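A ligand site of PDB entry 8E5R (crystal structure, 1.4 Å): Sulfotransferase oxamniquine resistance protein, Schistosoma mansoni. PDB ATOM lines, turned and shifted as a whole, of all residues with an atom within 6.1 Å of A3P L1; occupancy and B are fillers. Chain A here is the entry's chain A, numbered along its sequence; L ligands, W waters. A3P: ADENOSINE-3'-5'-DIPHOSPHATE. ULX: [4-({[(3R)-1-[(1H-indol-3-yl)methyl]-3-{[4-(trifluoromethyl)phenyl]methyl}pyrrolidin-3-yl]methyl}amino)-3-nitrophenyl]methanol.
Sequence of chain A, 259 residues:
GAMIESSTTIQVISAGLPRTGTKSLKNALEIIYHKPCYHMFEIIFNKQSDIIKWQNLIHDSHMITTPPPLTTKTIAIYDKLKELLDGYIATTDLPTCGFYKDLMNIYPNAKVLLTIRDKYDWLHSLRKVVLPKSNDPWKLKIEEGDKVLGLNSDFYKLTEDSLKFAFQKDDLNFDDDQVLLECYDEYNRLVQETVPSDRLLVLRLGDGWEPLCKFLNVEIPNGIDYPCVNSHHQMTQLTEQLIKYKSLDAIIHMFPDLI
An oxygen (O2P) of A3P L1 sits at hydrogen-bond distance from the side-chain hydroxyl of Ser 125 (2.6 Å). N of Thr 22 sits at hydrogen-bond distance from O4P of A3P L1. OG1 of Thr 22 is in hydrogen-bond range of O4P of A3P L1 (2.7 Å). The side-chain hydroxyl (OG) of Ser 24 is in hydrogen-bond range of a nitrogen (N7) of A3P L1, at 2.7 Å. The backbone NH (N) of Arg 19 lies within hydrogen-bond range of an oxygen (O4P) of A3P L1 (2.8 Å). The guanidinium group (NH1) of Arg 19 lies within salt-bridge range of an oxygen (O6P) of A3P L1, at 2.8 Å. The guanidinium group (NH2) of Arg 117 is in salt-bridge range of an oxygen (O1P) of A3P L1 (2.8 Å). The backbone NH (N) of Lys 23 lies within hydrogen-bond range of an oxygen (O5P) of A3P L1 (2.9 Å). O5' of A3P L1 is in hydrogen-bond range of N of Gly 21 (2.9 Å). N6 of A3P L1 is in hydrogen-bond range of O of Pro 227 (3.0 Å). The backbone NH (N) of His 232 is in hydrogen-bond range of an oxygen (O2P) of A3P L1. An oxygen (O5P) of A3P L1 is in hydrogen-bond range of the side-chain amide nitrogen of Asn 230 (3.1 Å). The backbone NH of Thr 20 sits at hydrogen-bond distance from an oxygen (O4P) of A3P L1, at 3.1 Å. The side-chain amide nitrogen (ND2) of Asn 230 lies within hydrogen-bond range of an oxygen (O9) of ULX L2. O9 of ULX L2 lies close to NE2 of His 39 (3.4 Å).
An oxygen (O6P) of A3P L1 sits at hydrogen-bond distance from an oxygen (O9) of ULX L2.
OG of Ser 125 sits at hydrogen-bond distance from NE of Arg 19. A ring nitrogen (NE2) of His 39 sits at hydrogen-bond distance from the side-chain hydroxyl of Thr 22 (2.9 Å). The side-chain hydroxyl (OG) of Ser 24 lies within hydrogen-bond range of the backbone carbonyl oxygen (O) of Pro 227 (3.2 Å). The side-chain hydroxyl (OG) of Ser 24 is in hydrogen-bond range of the backbone NH (N) of Val 229. NH1 of Arg 117 lies within hydrogen-bond range of O of Arg 19 (2.9 Å). NH2 of Arg 19 sits at hydrogen-bond distance from O of Asn 230 (2.8 Å). The backbone NH (N) of Lys 23 lies within hydrogen-bond range of a ring nitrogen (NE2) of His 39 (3.5 Å). The side-chain hydroxyl (OG1) of Thr 20 sits at hydrogen-bond distance from the backbone carbonyl oxygen (O) of Leu 17, 2.6 Å away.
C of Pro 18 touches O4P of A3P L1, at 3.9 Å. CD2 of Leu 205 touches C4 of A3P L1 (3.7 Å). N of Gly 206 touches N1 of A3P L1 (3.8 Å). CD2 of Tyr 226 touches N6 of A3P L1, 3.9 Å away. CAS 228 touches A3P L1. O of Val 229 touches C8 of A3P L1, at 3.4 Å. Ser 231 touches A3P L1 (CA to O3P, 3.4 Å). The nearest printed residue that does not touch A3P L1 is Leu 17 (4.3 Å).
Water W6 lies within hydrogen-bond range of an oxygen (O5P) of A3P L1 (2.7 Å), the backbone NH (N) of Ser 24 (2.9 Å), the backbone carbonyl oxygen (O) of Val 229 (2.9 Å) and the backbone NH (N) of Lys 23 (3.4 Å). Water W1 lies within hydrogen-bond range of an oxygen (O1P) of A3P L1 (2.7 Å) and the backbone carbonyl oxygen of Asp 121 (2.9 Å).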
ATOM      1  N   LEU A  17      32.769  22.492  -5.350  1.00  0.00           N
ATOM      2  CA  LEU A  17      33.594  22.873  -4.206  1.00  0.00           C
ATOM      3  C   LEU A  17      32.997  22.350  -2.889  1.00  0.00           C
ATOM      4  O   LEU A  17      31.819  21.999  -2.818  1.00  0.00           O
ATOM      5  CB  LEU A  17      33.681  24.398  -4.150  1.00  0.00           C
ATOM      6  CG  LEU A  17      34.483  25.063  -5.264  1.00  0.00           C
ATOM      7  CD1 LEU A  17      34.162  26.543  -5.352  1.00  0.00           C
ATOM      8  CD2 LEU A  17      35.991  24.828  -5.078  1.00  0.00           C
ATOM      9  N   PRO A  18      33.794  22.294  -1.826  1.00  0.00           N
ATOM     10  CA  PRO A  18      33.240  21.841  -0.530  1.00  0.00           C
ATOM     11  C   PRO A  18      32.044  22.690  -0.137  1.00  0.00           C
ATOM     12  O   PRO A  18      31.964  23.876  -0.457  1.00  0.00           O
ATOM     13  CB  PRO A  18      34.412  22.052   0.444  1.00  0.00           C
ATOM     14  CG  PRO A  18      35.445  22.809  -0.317  1.00  0.00           C
ATOM     15  CD  PRO A  18      35.234  22.529  -1.756  1.00  0.00           C
ATOM     16  N   ARG A  19      31.096  22.058   0.556  1.00  0.00           N
ATOM     17  CA  ARG A  19      29.855  22.697   1.022  1.00  0.00           C
ATOM     18  C   ARG A  19      28.848  22.949  -0.104  1.00  0.00           C
ATOM     19  O   ARG A  19      28.006  23.837   0.023  1.00  0.00           O
ATOM     20  CB  ARG A  19      30.090  23.963   1.865  1.00  0.00           C
ATOM     21  CG  ARG A  19      31.146  23.797   2.959  1.00  0.00           C
ATOM     22  CD  ARG A  19      30.877  22.557   3.836  1.00  0.00           C
ATOM     23  NE  ARG A  19      29.639  22.652   4.596  1.00  0.00           N
ATOM     24  CZ  ARG A  19      29.105  21.651   5.292  1.00  0.00           C
ATOM     25  NH1 ARG A  19      29.672  20.448   5.332  1.00  0.00           N
ATOM     26  NH2 ARG A  19      27.999  21.864   6.000  1.00  0.00           N
ATOM     27  N   THR A  20      28.921  22.171  -1.175  1.00  0.00           N
ATOM     28  CA  THR A  20      27.944  22.237  -2.266  1.00  0.00           C
ATOM     29  C   THR A  20      27.185  20.919  -2.431  1.00  0.00           C
ATOM     30  O   THR A  20      26.679  20.638  -3.512  1.00  0.00           O
ATOM     31  CB  THR A  20      28.580  22.664  -3.595  1.00  0.00           C
ATOM     32  OG1 THR A  20      29.536  21.678  -4.027  1.00  0.00           O
ATOM     33  CG2 THR A  20      29.249  24.037  -3.509  1.00  0.00           C
ATOM     34  N   GLY A  21      27.090  20.125  -1.376  1.00  0.00           N
ATOM     35  CA  GLY A  21      26.472  18.820  -1.481  1.00  0.00           C
ATOM     36  C   GLY A  21      27.397  17.686  -1.891  1.00  0.00           C
ATOM     37  O   GLY A  21      26.916  16.669  -2.402  1.00  0.00           O
ATOM     38  N   THR A  22      28.716  17.822  -1.675  1.00  0.00           N
ATOM     39  CA  THR A  22      29.651  16.785  -2.122  1.00  0.00           C
ATOM     40  C   THR A  22      29.464  15.467  -1.362  1.00  0.00           C
ATOM     41  O   THR A  22      29.624  14.389  -1.939  1.00  0.00           O
ATOM     42  CB  THR A  22      31.107  17.255  -2.024  1.00  0.00           C
ATOM     43  OG1 THR A  22      31.451  17.452  -0.640  1.00  0.00           O
ATOM     44  CG2 THR A  22      31.345  18.548  -2.816  1.00  0.00           C
ATOM     45  N   LYS A  23      29.166  15.521  -0.058  1.00  0.00           N
ATOM     46  CA  LYS A  23      29.021  14.268   0.673  1.00  0.00           C
ATOM     47  C   LYS A  23      27.759  13.519   0.263  1.00  0.00           C
ATOM     48  O   LYS A  23      27.777  12.290   0.090  1.00  0.00           O
ATOM     49  CB  LYS A  23      29.118  14.473   2.185  1.00  0.00           C
ATOM     50  CG  LYS A  23      29.064  13.168   2.982  1.00  0.00           C
ATOM     51  CD  LYS A  23      30.243  12.260   2.663  1.00  0.00           C
ATOM     52  CE  LYS A  23      30.470  11.189   3.735  1.00  0.00           C
ATOM     53  NZ  LYS A  23      29.377  10.185   3.837  1.00  0.00           N
ATOM     54  N   SER A  24      26.647  14.242   0.095  1.00  0.00           N
ATOM     55  CA  SER A  24      25.443  13.618  -0.418  1.00  0.00           C
ATOM     56  C   SER A  24      25.702  12.983  -1.782  1.00  0.00           C
ATOM     57  O   SER A  24      25.241  11.863  -2.052  1.00  0.00           O
ATOM     58  CB  SER A  24      24.333  14.656  -0.536  1.00  0.00           C
ATOM     59  OG  SER A  24      23.880  15.026   0.750  1.00  0.00           O
ATOM     60  N   HIS A  39      36.486  11.417  -1.474  1.00  0.00           N
ATOM     61  CA  HIS A  39      35.934  12.579  -0.791  1.00  0.00           C
ATOM     62  C   HIS A  39      36.922  12.884   0.326  1.00  0.00           C
ATOM     63  O   HIS A  39      37.685  12.007   0.738  1.00  0.00           O
ATOM     64  CB  HIS A  39      34.564  12.236  -0.191  1.00  0.00           C
ATOM     65  CG  HIS A  39      33.825  13.410   0.368  1.00  0.00           C
ATOM     66  ND1 HIS A  39      33.958  13.831   1.673  1.00  0.00           N
ATOM     67  CD2 HIS A  39      32.888  14.216  -0.196  1.00  0.00           C
ATOM     68  CE1 HIS A  39      33.162  14.866   1.883  1.00  0.00           C
ATOM     69  NE2 HIS A  39      32.497  15.114   0.768  1.00  0.00           N
ATOM     70  N   ASP A  93      34.857  16.616  -3.964  1.00  0.00           N
ATOM     71  CA  ASP A  93      35.355  17.410  -2.840  1.00  0.00           C
ATOM     72  C   ASP A  93      36.845  17.716  -2.981  1.00  0.00           C
ATOM     73  O   ASP A  93      37.511  17.247  -3.912  1.00  0.00           O
ATOM     74  CB  ASP A  93      35.021  16.689  -1.532  1.00  0.00           C
ATOM     75  CG  ASP A  93      35.223  17.536  -0.295  1.00  0.00           C
ATOM     76  OD1 ASP A  93      35.258  18.780  -0.380  1.00  0.00           O
ATOM     77  OD2 ASP A  93      35.274  16.919   0.789  1.00  0.00           O
ATOM     78  N   ARG A 117      25.532  26.282  -5.651  1.00  0.00           N
ATOM     79  CA  ARG A 117      24.487  26.822  -4.783  1.00  0.00           C
ATOM     80  C   ARG A 117      24.675  28.330  -4.658  1.00  0.00           C
ATOM     81  O   ARG A 117      25.658  28.911  -5.119  1.00  0.00           O
ATOM     82  CB  ARG A 117      24.499  26.141  -3.410  1.00  0.00           C
ATOM     83  CG  ARG A 117      25.683  26.567  -2.560  1.00  0.00           C
ATOM     84  CD  ARG A 117      25.809  25.755  -1.271  1.00  0.00           C
ATOM     85  NE  ARG A 117      24.693  25.969  -0.352  1.00  0.00           N
ATOM     86  CZ  ARG A 117      24.694  25.538   0.900  1.00  0.00           C
ATOM     87  NH1 ARG A 117      25.740  24.932   1.432  1.00  0.00           N
ATOM     88  NH2 ARG A 117      23.595  25.724   1.648  1.00  0.00           N
ATOM     89  N   ASP A 121      24.975  31.464   0.928  1.00  0.00           N
ATOM     90  CA  ASP A 121      24.737  30.201   1.630  1.00  0.00           C
ATOM     91  C   ASP A 121      26.013  29.363   1.691  1.00  0.00           C
ATOM     92  O   ASP A 121      26.335  28.746   2.712  1.00  0.00           O
ATOM     93  CB  ASP A 121      23.664  29.387   0.892  1.00  0.00           C
ATOM     94  CG  ASP A 121      22.258  29.925   1.105  1.00  0.00           C
ATOM     95  OD1 ASP A 121      22.076  30.830   1.944  1.00  0.00           O
ATOM     96  OD2 ASP A 121      21.326  29.445   0.427  1.00  0.00           O
ATOM     97  N   HIS A 124      28.507  30.989   4.179  1.00  0.00           N
ATOM     98  CA  HIS A 124      28.061  30.754   5.549  1.00  0.00           C
ATOM     99  C   HIS A 124      28.399  29.345   5.993  1.00  0.00           C
ATOM    100  O   HIS A 124      28.915  29.118   7.097  1.00  0.00           O
ATOM    101  CB  HIS A 124      26.541  30.978   5.630  1.00  0.00           C
ATOM    102  CG  HIS A 124      25.940  30.695   6.973  1.00  0.00           C
ATOM    103  ND1 HIS A 124      26.045  31.581   8.021  1.00  0.00           N
ATOM    104  CD2 HIS A 124      25.192  29.653   7.425  1.00  0.00           C
ATOM    105  CE1 HIS A 124      25.413  31.088   9.072  1.00  0.00           C
ATOM    106  NE2 HIS A 124      24.878  29.927   8.734  1.00  0.00           N
ATOM    107  N   SER A 125      28.129  28.370   5.121  1.00  0.00           N
ATOM    108  CA  SER A 125      28.406  26.965   5.422  1.00  0.00           C
ATOM    109  C   SER A 125      29.904  26.733   5.548  1.00  0.00           C
ATOM    110  O   SER A 125      30.370  26.054   6.476  1.00  0.00           O
ATOM    111  CB  SER A 125      27.836  26.125   4.281  1.00  0.00           C
ATOM    112  OG  SER A 125      27.860  24.758   4.596  1.00  0.00           O
ATOM    113  N   VAL A 129      32.186  25.310   8.999  1.00  0.00           N
ATOM    114  CA  VAL A 129      32.712  23.913   8.983  1.00  0.00           C
ATOM    115  C   VAL A 129      34.150  23.802   8.467  1.00  0.00           C
ATOM    116  O   VAL A 129      34.932  23.087   9.107  1.00  0.00           O
ATOM    117  CB  VAL A 129      31.781  23.070   8.085  1.00  0.00           C
ATOM    118  CG1 VAL A 129      32.322  21.673   7.822  1.00  0.00           C
ATOM    119  CG2 VAL A 129      30.356  23.003   8.619  1.00  0.00           C
ATOM    120  N   VAL A 130      34.499  24.520   7.397  1.00  0.00           N
ATOM    121  CA  VAL A 130      35.771  24.284   6.725  1.00  0.00           C
ATOM    122  C   VAL A 130      36.807  25.358   7.052  1.00  0.00           C
ATOM    123  O   VAL A 130      37.968  25.044   7.328  1.00  0.00           O
ATOM    124  CB  VAL A 130      35.564  24.167   5.195  1.00  0.00           C
ATOM    125  CG1 VAL A 130      36.888  23.836   4.499  1.00  0.00           C
ATOM    126  CG2 VAL A 130      34.529  23.104   4.884  1.00  0.00           C
ATOM    127  N   LEU A 205      21.603  22.077  -5.447  1.00  0.00           N
ATOM    128  CA  LEU A 205      21.097  21.383  -4.271  1.00  0.00           C
ATOM    129  C   LEU A 205      19.589  21.192  -4.368  1.00  0.00           C
ATOM    130  O   LEU A 205      18.859  22.134  -4.678  1.00  0.00           O
ATOM    131  CB  LEU A 205      21.425  22.170  -2.999  1.00  0.00           C
ATOM    132  CG  LEU A 205      22.883  22.249  -2.560  1.00  0.00           C
ATOM    133  CD1 LEU A 205      23.043  23.162  -1.341  1.00  0.00           C
ATOM    134  CD2 LEU A 205      23.435  20.852  -2.268  1.00  0.00           C
ATOM    135  N   GLY A 206      19.144  19.970  -4.089  1.00  0.00           N
ATOM    136  CA  GLY A 206      17.740  19.621  -4.182  1.00  0.00           C
ATOM    137  C   GLY A 206      17.314  18.992  -5.494  1.00  0.00           C
ATOM    138  O   GLY A 206      16.142  18.596  -5.607  1.00  0.00           O
ATOM    139  N   TYR A 226      17.194  10.428  -2.294  1.00  0.00           N
ATOM    140  CA  TYR A 226      18.483  11.043  -2.569  1.00  0.00           C
ATOM    141  C   TYR A 226      19.079  11.529  -1.251  1.00  0.00           C
ATOM    142  O   TYR A 226      18.376  12.147  -0.437  1.00  0.00           O
ATOM    143  CB  TYR A 226      18.348  12.204  -3.544  1.00  0.00           C
ATOM    144  CG  TYR A 226      19.711  12.746  -3.951  1.00  0.00           C
ATOM    145  CD1 TYR A 226      20.386  12.219  -5.046  1.00  0.00           C
ATOM    146  CD2 TYR A 226      20.314  13.784  -3.241  1.00  0.00           C
ATOM    147  CE1 TYR A 226      21.617  12.716  -5.422  1.00  0.00           C
ATOM    148  CE2 TYR A 226      21.545  14.286  -3.609  1.00  0.00           C
ATOM    149  CZ  TYR A 226      22.192  13.730  -4.708  1.00  0.00           C
ATOM    150  OH  TYR A 226      23.443  14.227  -5.073  1.00  0.00           O
ATOM    151  N   PRO A 227      20.369  11.257  -0.992  1.00  0.00           N
ATOM    152  CA  PRO A 227      20.980  11.588   0.304  1.00  0.00           C
ATOM    153  C   PRO A 227      20.924  13.061   0.666  1.00  0.00           C
ATOM    154  O   PRO A 227      21.064  13.933  -0.202  1.00  0.00           O
ATOM    155  CB  PRO A 227      22.442  11.169   0.134  1.00  0.00           C
ATOM    156  CG  PRO A 227      22.400  10.148  -0.936  1.00  0.00           C
ATOM    157  CD  PRO A 227      21.318  10.580  -1.878  1.00  0.00           C
ATOM    158  N   CAS A 228      20.711  13.342   1.946  1.00  0.00           N
ATOM    159  CA  CAS A 228      20.778  14.691   2.455  1.00  0.00           C
ATOM    160  CB  CAS A 228      19.373  15.224   2.718  1.00  0.00           C
ATOM    161  C   CAS A 228      21.559  14.589   3.749  1.00  0.00           C
ATOM    162  O   CAS A 228      21.013  14.237   4.817  1.00  0.00           O
ATOM    163  SG  CAS A 228      19.509  16.959   3.232  1.00  0.00           S
ATOM    164 AS   CAS A 228      19.370  17.086   5.481  1.00  0.00          AS
ATOM    165  CE1 CAS A 228      21.181  17.178   6.237  1.00  0.00           C
ATOM    166  CE2 CAS A 228      18.449  18.754   5.956  1.00  0.00           C
ATOM    167  N   VAL A 229      22.737  14.945   3.686  1.00  0.00           N
ATOM    168  CA  VAL A 229      23.705  14.740   4.806  1.00  0.00           C
ATOM    169  C   VAL A 229      24.736  15.871   4.850  1.00  0.00           C
ATOM    170  O   VAL A 229      24.840  16.611   3.851  1.00  0.00           O
ATOM    171  CB  VAL A 229      24.408  13.371   4.700  1.00  0.00           C
ATOM    172  CG1 VAL A 229      23.413  12.223   4.668  1.00  0.00           C
ATOM    173  CG2 VAL A 229      25.351  13.299   3.517  1.00  0.00           C
ATOM    174  N   ASN A 230      25.438  16.014   5.979  1.00  0.00           N
ATOM    175  CA  ASN A 230      26.560  16.983   6.111  1.00  0.00           C
ATOM    176  C   ASN A 230      26.084  18.436   6.243  1.00  0.00           C
ATOM    177  O   ASN A 230      26.810  19.327   5.815  1.00  0.00           O
ATOM    178  CB  ASN A 230      27.608  16.800   5.007  1.00  0.00           C
ATOM    179  CG  ASN A 230      29.023  17.041   5.462  1.00  0.00           C
ATOM    180  OD1 ASN A 230      29.298  17.101   6.649  1.00  0.00           O
ATOM    181  ND2 ASN A 230      29.933  17.178   4.513  1.00  0.00           N
ATOM    182  N   SER A 231      24.912  18.653   6.843  1.00  0.00           N
ATOM    183  CA  SER A 231      24.463  20.045   7.108  1.00  0.00           C
ATOM    184  C   SER A 231      25.435  20.672   8.119  1.00  0.00           C
ATOM    185  O   SER A 231      26.031  19.931   8.906  1.00  0.00           O
ATOM    186  CB  SER A 231      23.045  20.076   7.627  1.00  0.00           C
ATOM    187  OG  SER A 231      22.967  19.584   8.953  1.00  0.00           O
ATOM    188  N   HIS A 232      25.575  21.995   8.100  1.00  0.00           N
ATOM    189  CA  HIS A 232      26.434  22.593   9.118  1.00  0.00           C
ATOM    190  C   HIS A 232      25.911  22.322  10.524  1.00  0.00           C
ATOM    191  O   HIS A 232      26.702  22.173  11.457  1.00  0.00           O
ATOM    192  CB  HIS A 232      26.720  24.071   8.882  1.00  0.00           C
ATOM    193  CG  HIS A 232      25.532  24.963   9.093  1.00  0.00           C
ATOM    194  ND1 HIS A 232      25.132  25.390  10.342  1.00  0.00           N
ATOM    195  CD2 HIS A 232      24.687  25.531   8.205  1.00  0.00           C
ATOM    196  CE1 HIS A 232      24.083  26.179  10.215  1.00  0.00           C
ATOM    197  NE2 HIS A 232      23.792  26.282   8.926  1.00  0.00           N
ATOM    198  N   HIS A 233      24.601  22.201  10.688  1.00  0.00           N
ATOM    199  CA  HIS A 233      24.054  21.864  11.995  1.00  0.00           C
ATOM    200  C   HIS A 233      24.527  20.492  12.437  1.00  0.00           C
ATOM    201  O   HIS A 233      24.883  20.286  13.601  1.00  0.00           O
ATOM    202  CB  HIS A 233      22.518  21.865  11.932  1.00  0.00           C
ATOM    203  CG  HIS A 233      21.919  23.223  11.747  1.00  0.00           C
ATOM    204  ND1 HIS A 233      22.066  24.242  12.676  1.00  0.00           N
ATOM    205  CD2 HIS A 233      21.173  23.745  10.744  1.00  0.00           C
ATOM    206  CE1 HIS A 233      21.431  25.319  12.244  1.00  0.00           C
ATOM    207  NE2 HIS A 233      20.876  25.040  11.080  1.00  0.00           N
HETATM  208  P1  A3P L   1      24.527  23.675   4.873  1.00  0.00           P
HETATM  209  O1P A3P L   1      24.144  25.030   4.357  1.00  0.00           O
HETATM  210  O2P A3P L   1      25.812  23.627   5.618  1.00  0.00           O
HETATM  211  O3P A3P L   1      23.425  22.947   5.581  1.00  0.00           O
HETATM  212  P2  A3P L   1      29.248  19.204   1.489  1.00  0.00           P
HETATM  213  O4P A3P L   1      29.883  19.516   0.174  1.00  0.00           O
HETATM  214  O5P A3P L   1      28.826  17.782   1.680  1.00  0.00           O
HETATM  215  O6P A3P L   1      30.014  19.738   2.667  1.00  0.00           O
HETATM  216  O5' A3P L   1      27.884  20.029   1.438  1.00  0.00           O
HETATM  217  C5' A3P L   1      27.008  20.125   2.559  1.00  0.00           C
HETATM  218  C4' A3P L   1      25.972  21.205   2.295  1.00  0.00           C
HETATM  219  O4' A3P L   1      25.069  20.796   1.277  1.00  0.00           O
HETATM  220  C3' A3P L   1      25.135  21.466   3.524  1.00  0.00           C
HETATM  221  O3' A3P L   1      24.771  22.831   3.522  1.00  0.00           O
HETATM  222  C2' A3P L   1      23.956  20.547   3.302  1.00  0.00           C
HETATM  223  O2' A3P L   1      22.784  20.919   4.029  1.00  0.00           O
HETATM  224  C1' A3P L   1      23.749  20.695   1.818  1.00  0.00           C
HETATM  225  N9  A3P L   1      23.035  19.524   1.265  1.00  0.00           N
HETATM  226  C8  A3P L   1      23.512  18.277   1.204  1.00  0.00           C
HETATM  227  N7  A3P L   1      22.615  17.439   0.644  1.00  0.00           N
HETATM  228  C5  A3P L   1      21.531  18.152   0.340  1.00  0.00           C
HETATM  229  C6  A3P L   1      20.215  17.876  -0.272  1.00  0.00           C
HETATM  230  N6  A3P L   1      19.886  16.626  -0.674  1.00  0.00           N
HETATM  231  N1  A3P L   1      19.364  18.898  -0.407  1.00  0.00           N
HETATM  232  C2  A3P L   1      19.680  20.143   0.000  1.00  0.00           C
HETATM  233  N3  A3P L   1      20.862  20.470   0.558  1.00  0.00           N
HETATM  234  C4  A3P L   1      21.808  19.530   0.758  1.00  0.00           C
HETATM  235  C1  ULX L   2      33.543  19.109   4.775  1.00  0.00           C
HETATM  236  C10 ULX L   2      40.158  24.407  11.715  1.00  0.00           C
HETATM  237  C11 ULX L   2      37.643  20.447   8.438  1.00  0.00           C
HETATM  238  C12 ULX L   2      41.761  25.344  10.467  1.00  0.00           C
HETATM  239  C13 ULX L   2      33.943  15.601  10.861  1.00  0.00           C
HETATM  240  C14 ULX L   2      38.796  21.134   7.731  1.00  0.00           C
HETATM  241  C15 ULX L   2      39.677  21.601   8.867  1.00  0.00           C
HETATM  242  C16 ULX L   2      40.778  24.733   9.553  1.00  0.00           C
HETATM  243  C17 ULX L   2      37.515  21.165   9.772  1.00  0.00           C
HETATM  244  C18 ULX L   2      42.871  25.994   9.913  1.00  0.00           C
HETATM  245  C19 ULX L   2      43.000  26.049   8.530  1.00  0.00           C
HETATM  246  C2  ULX L   2      33.929  18.981   3.444  1.00  0.00           C
HETATM  247  C20 ULX L   2      42.066  25.457   7.675  1.00  0.00           C
HETATM  248  C21 ULX L   2      40.942  24.802   8.173  1.00  0.00           C
HETATM  249  C22 ULX L   2      38.000  18.981   8.587  1.00  0.00           C
HETATM  250  C23 ULX L   2      36.920  18.101   9.167  1.00  0.00           C
HETATM  251  C24 ULX L   2      36.773  18.008  10.538  1.00  0.00           C
HETATM  252  C25 ULX L   2      35.798  17.195  11.086  1.00  0.00           C
HETATM  253  C26 ULX L   2      34.984  16.469  10.242  1.00  0.00           C
HETATM  254  C27 ULX L   2      35.116  16.537   8.863  1.00  0.00           C
HETATM  255  C28 ULX L   2      36.090  17.356   8.323  1.00  0.00           C
HETATM  256  C3  ULX L   2      35.252  19.194   3.080  1.00  0.00           C
HETATM  257  C30 ULX L   2      36.394  20.601   7.567  1.00  0.00           C
HETATM  258  C4  ULX L   2      36.183  19.553   4.035  1.00  0.00           C
HETATM  259  C5  ULX L   2      35.809  19.686   5.362  1.00  0.00           C
HETATM  260  C6  ULX L   2      34.481  19.457   5.736  1.00  0.00           C
HETATM  261  C7  ULX L   2      32.935  18.598   2.376  1.00  0.00           C
HETATM  262  C8  ULX L   2      38.508  23.367   9.982  1.00  0.00           C
HETATM  263  C9  ULX L   2      39.738  24.126  10.409  1.00  0.00           C
HETATM  264  F14 ULX L   2      32.934  15.454  10.022  1.00  0.00           F
HETATM  265  F15 ULX L   2      34.449  14.414  11.127  1.00  0.00           F
HETATM  266  F16 ULX L   2      33.552  16.186  11.975  1.00  0.00           F
HETATM  267  N11 ULX L   2      41.335  25.113  11.716  1.00  0.00           N
HETATM  268  N12 ULX L   2      36.740  20.023   6.283  1.00  0.00           N
HETATM  269  N16 ULX L   2      38.765  21.914   9.981  1.00  0.00           N
HETATM  270  N17 ULX L   2      37.511  19.771   3.644  1.00  0.00           N
HETATM  271  O10 ULX L   2      37.880  19.578   2.319  1.00  0.00           O
HETATM  272  O11 ULX L   2      38.476  20.165   4.577  1.00  0.00           O
HETATM  273  O9  ULX L   2      31.985  17.664   2.904  1.00  0.00           O
HETATM  274  O   HOH W   1      24.499  27.685   4.668  1.00  0.00           O
HETATM  275  O   HOH W   2      21.102  24.588   3.955  1.00  0.00           O
HETATM  276  O   HOH W   3      21.709  23.554   7.349  1.00  0.00           O
HETATM  277  O   HOH W   4      20.393  23.113   1.596  1.00  0.00           O
HETATM  278  O   HOH W   5      16.546  18.855  -0.637  1.00  0.00           O
HETATM  279  O   HOH W   6      26.381  16.802   1.372  1.00  0.00           O
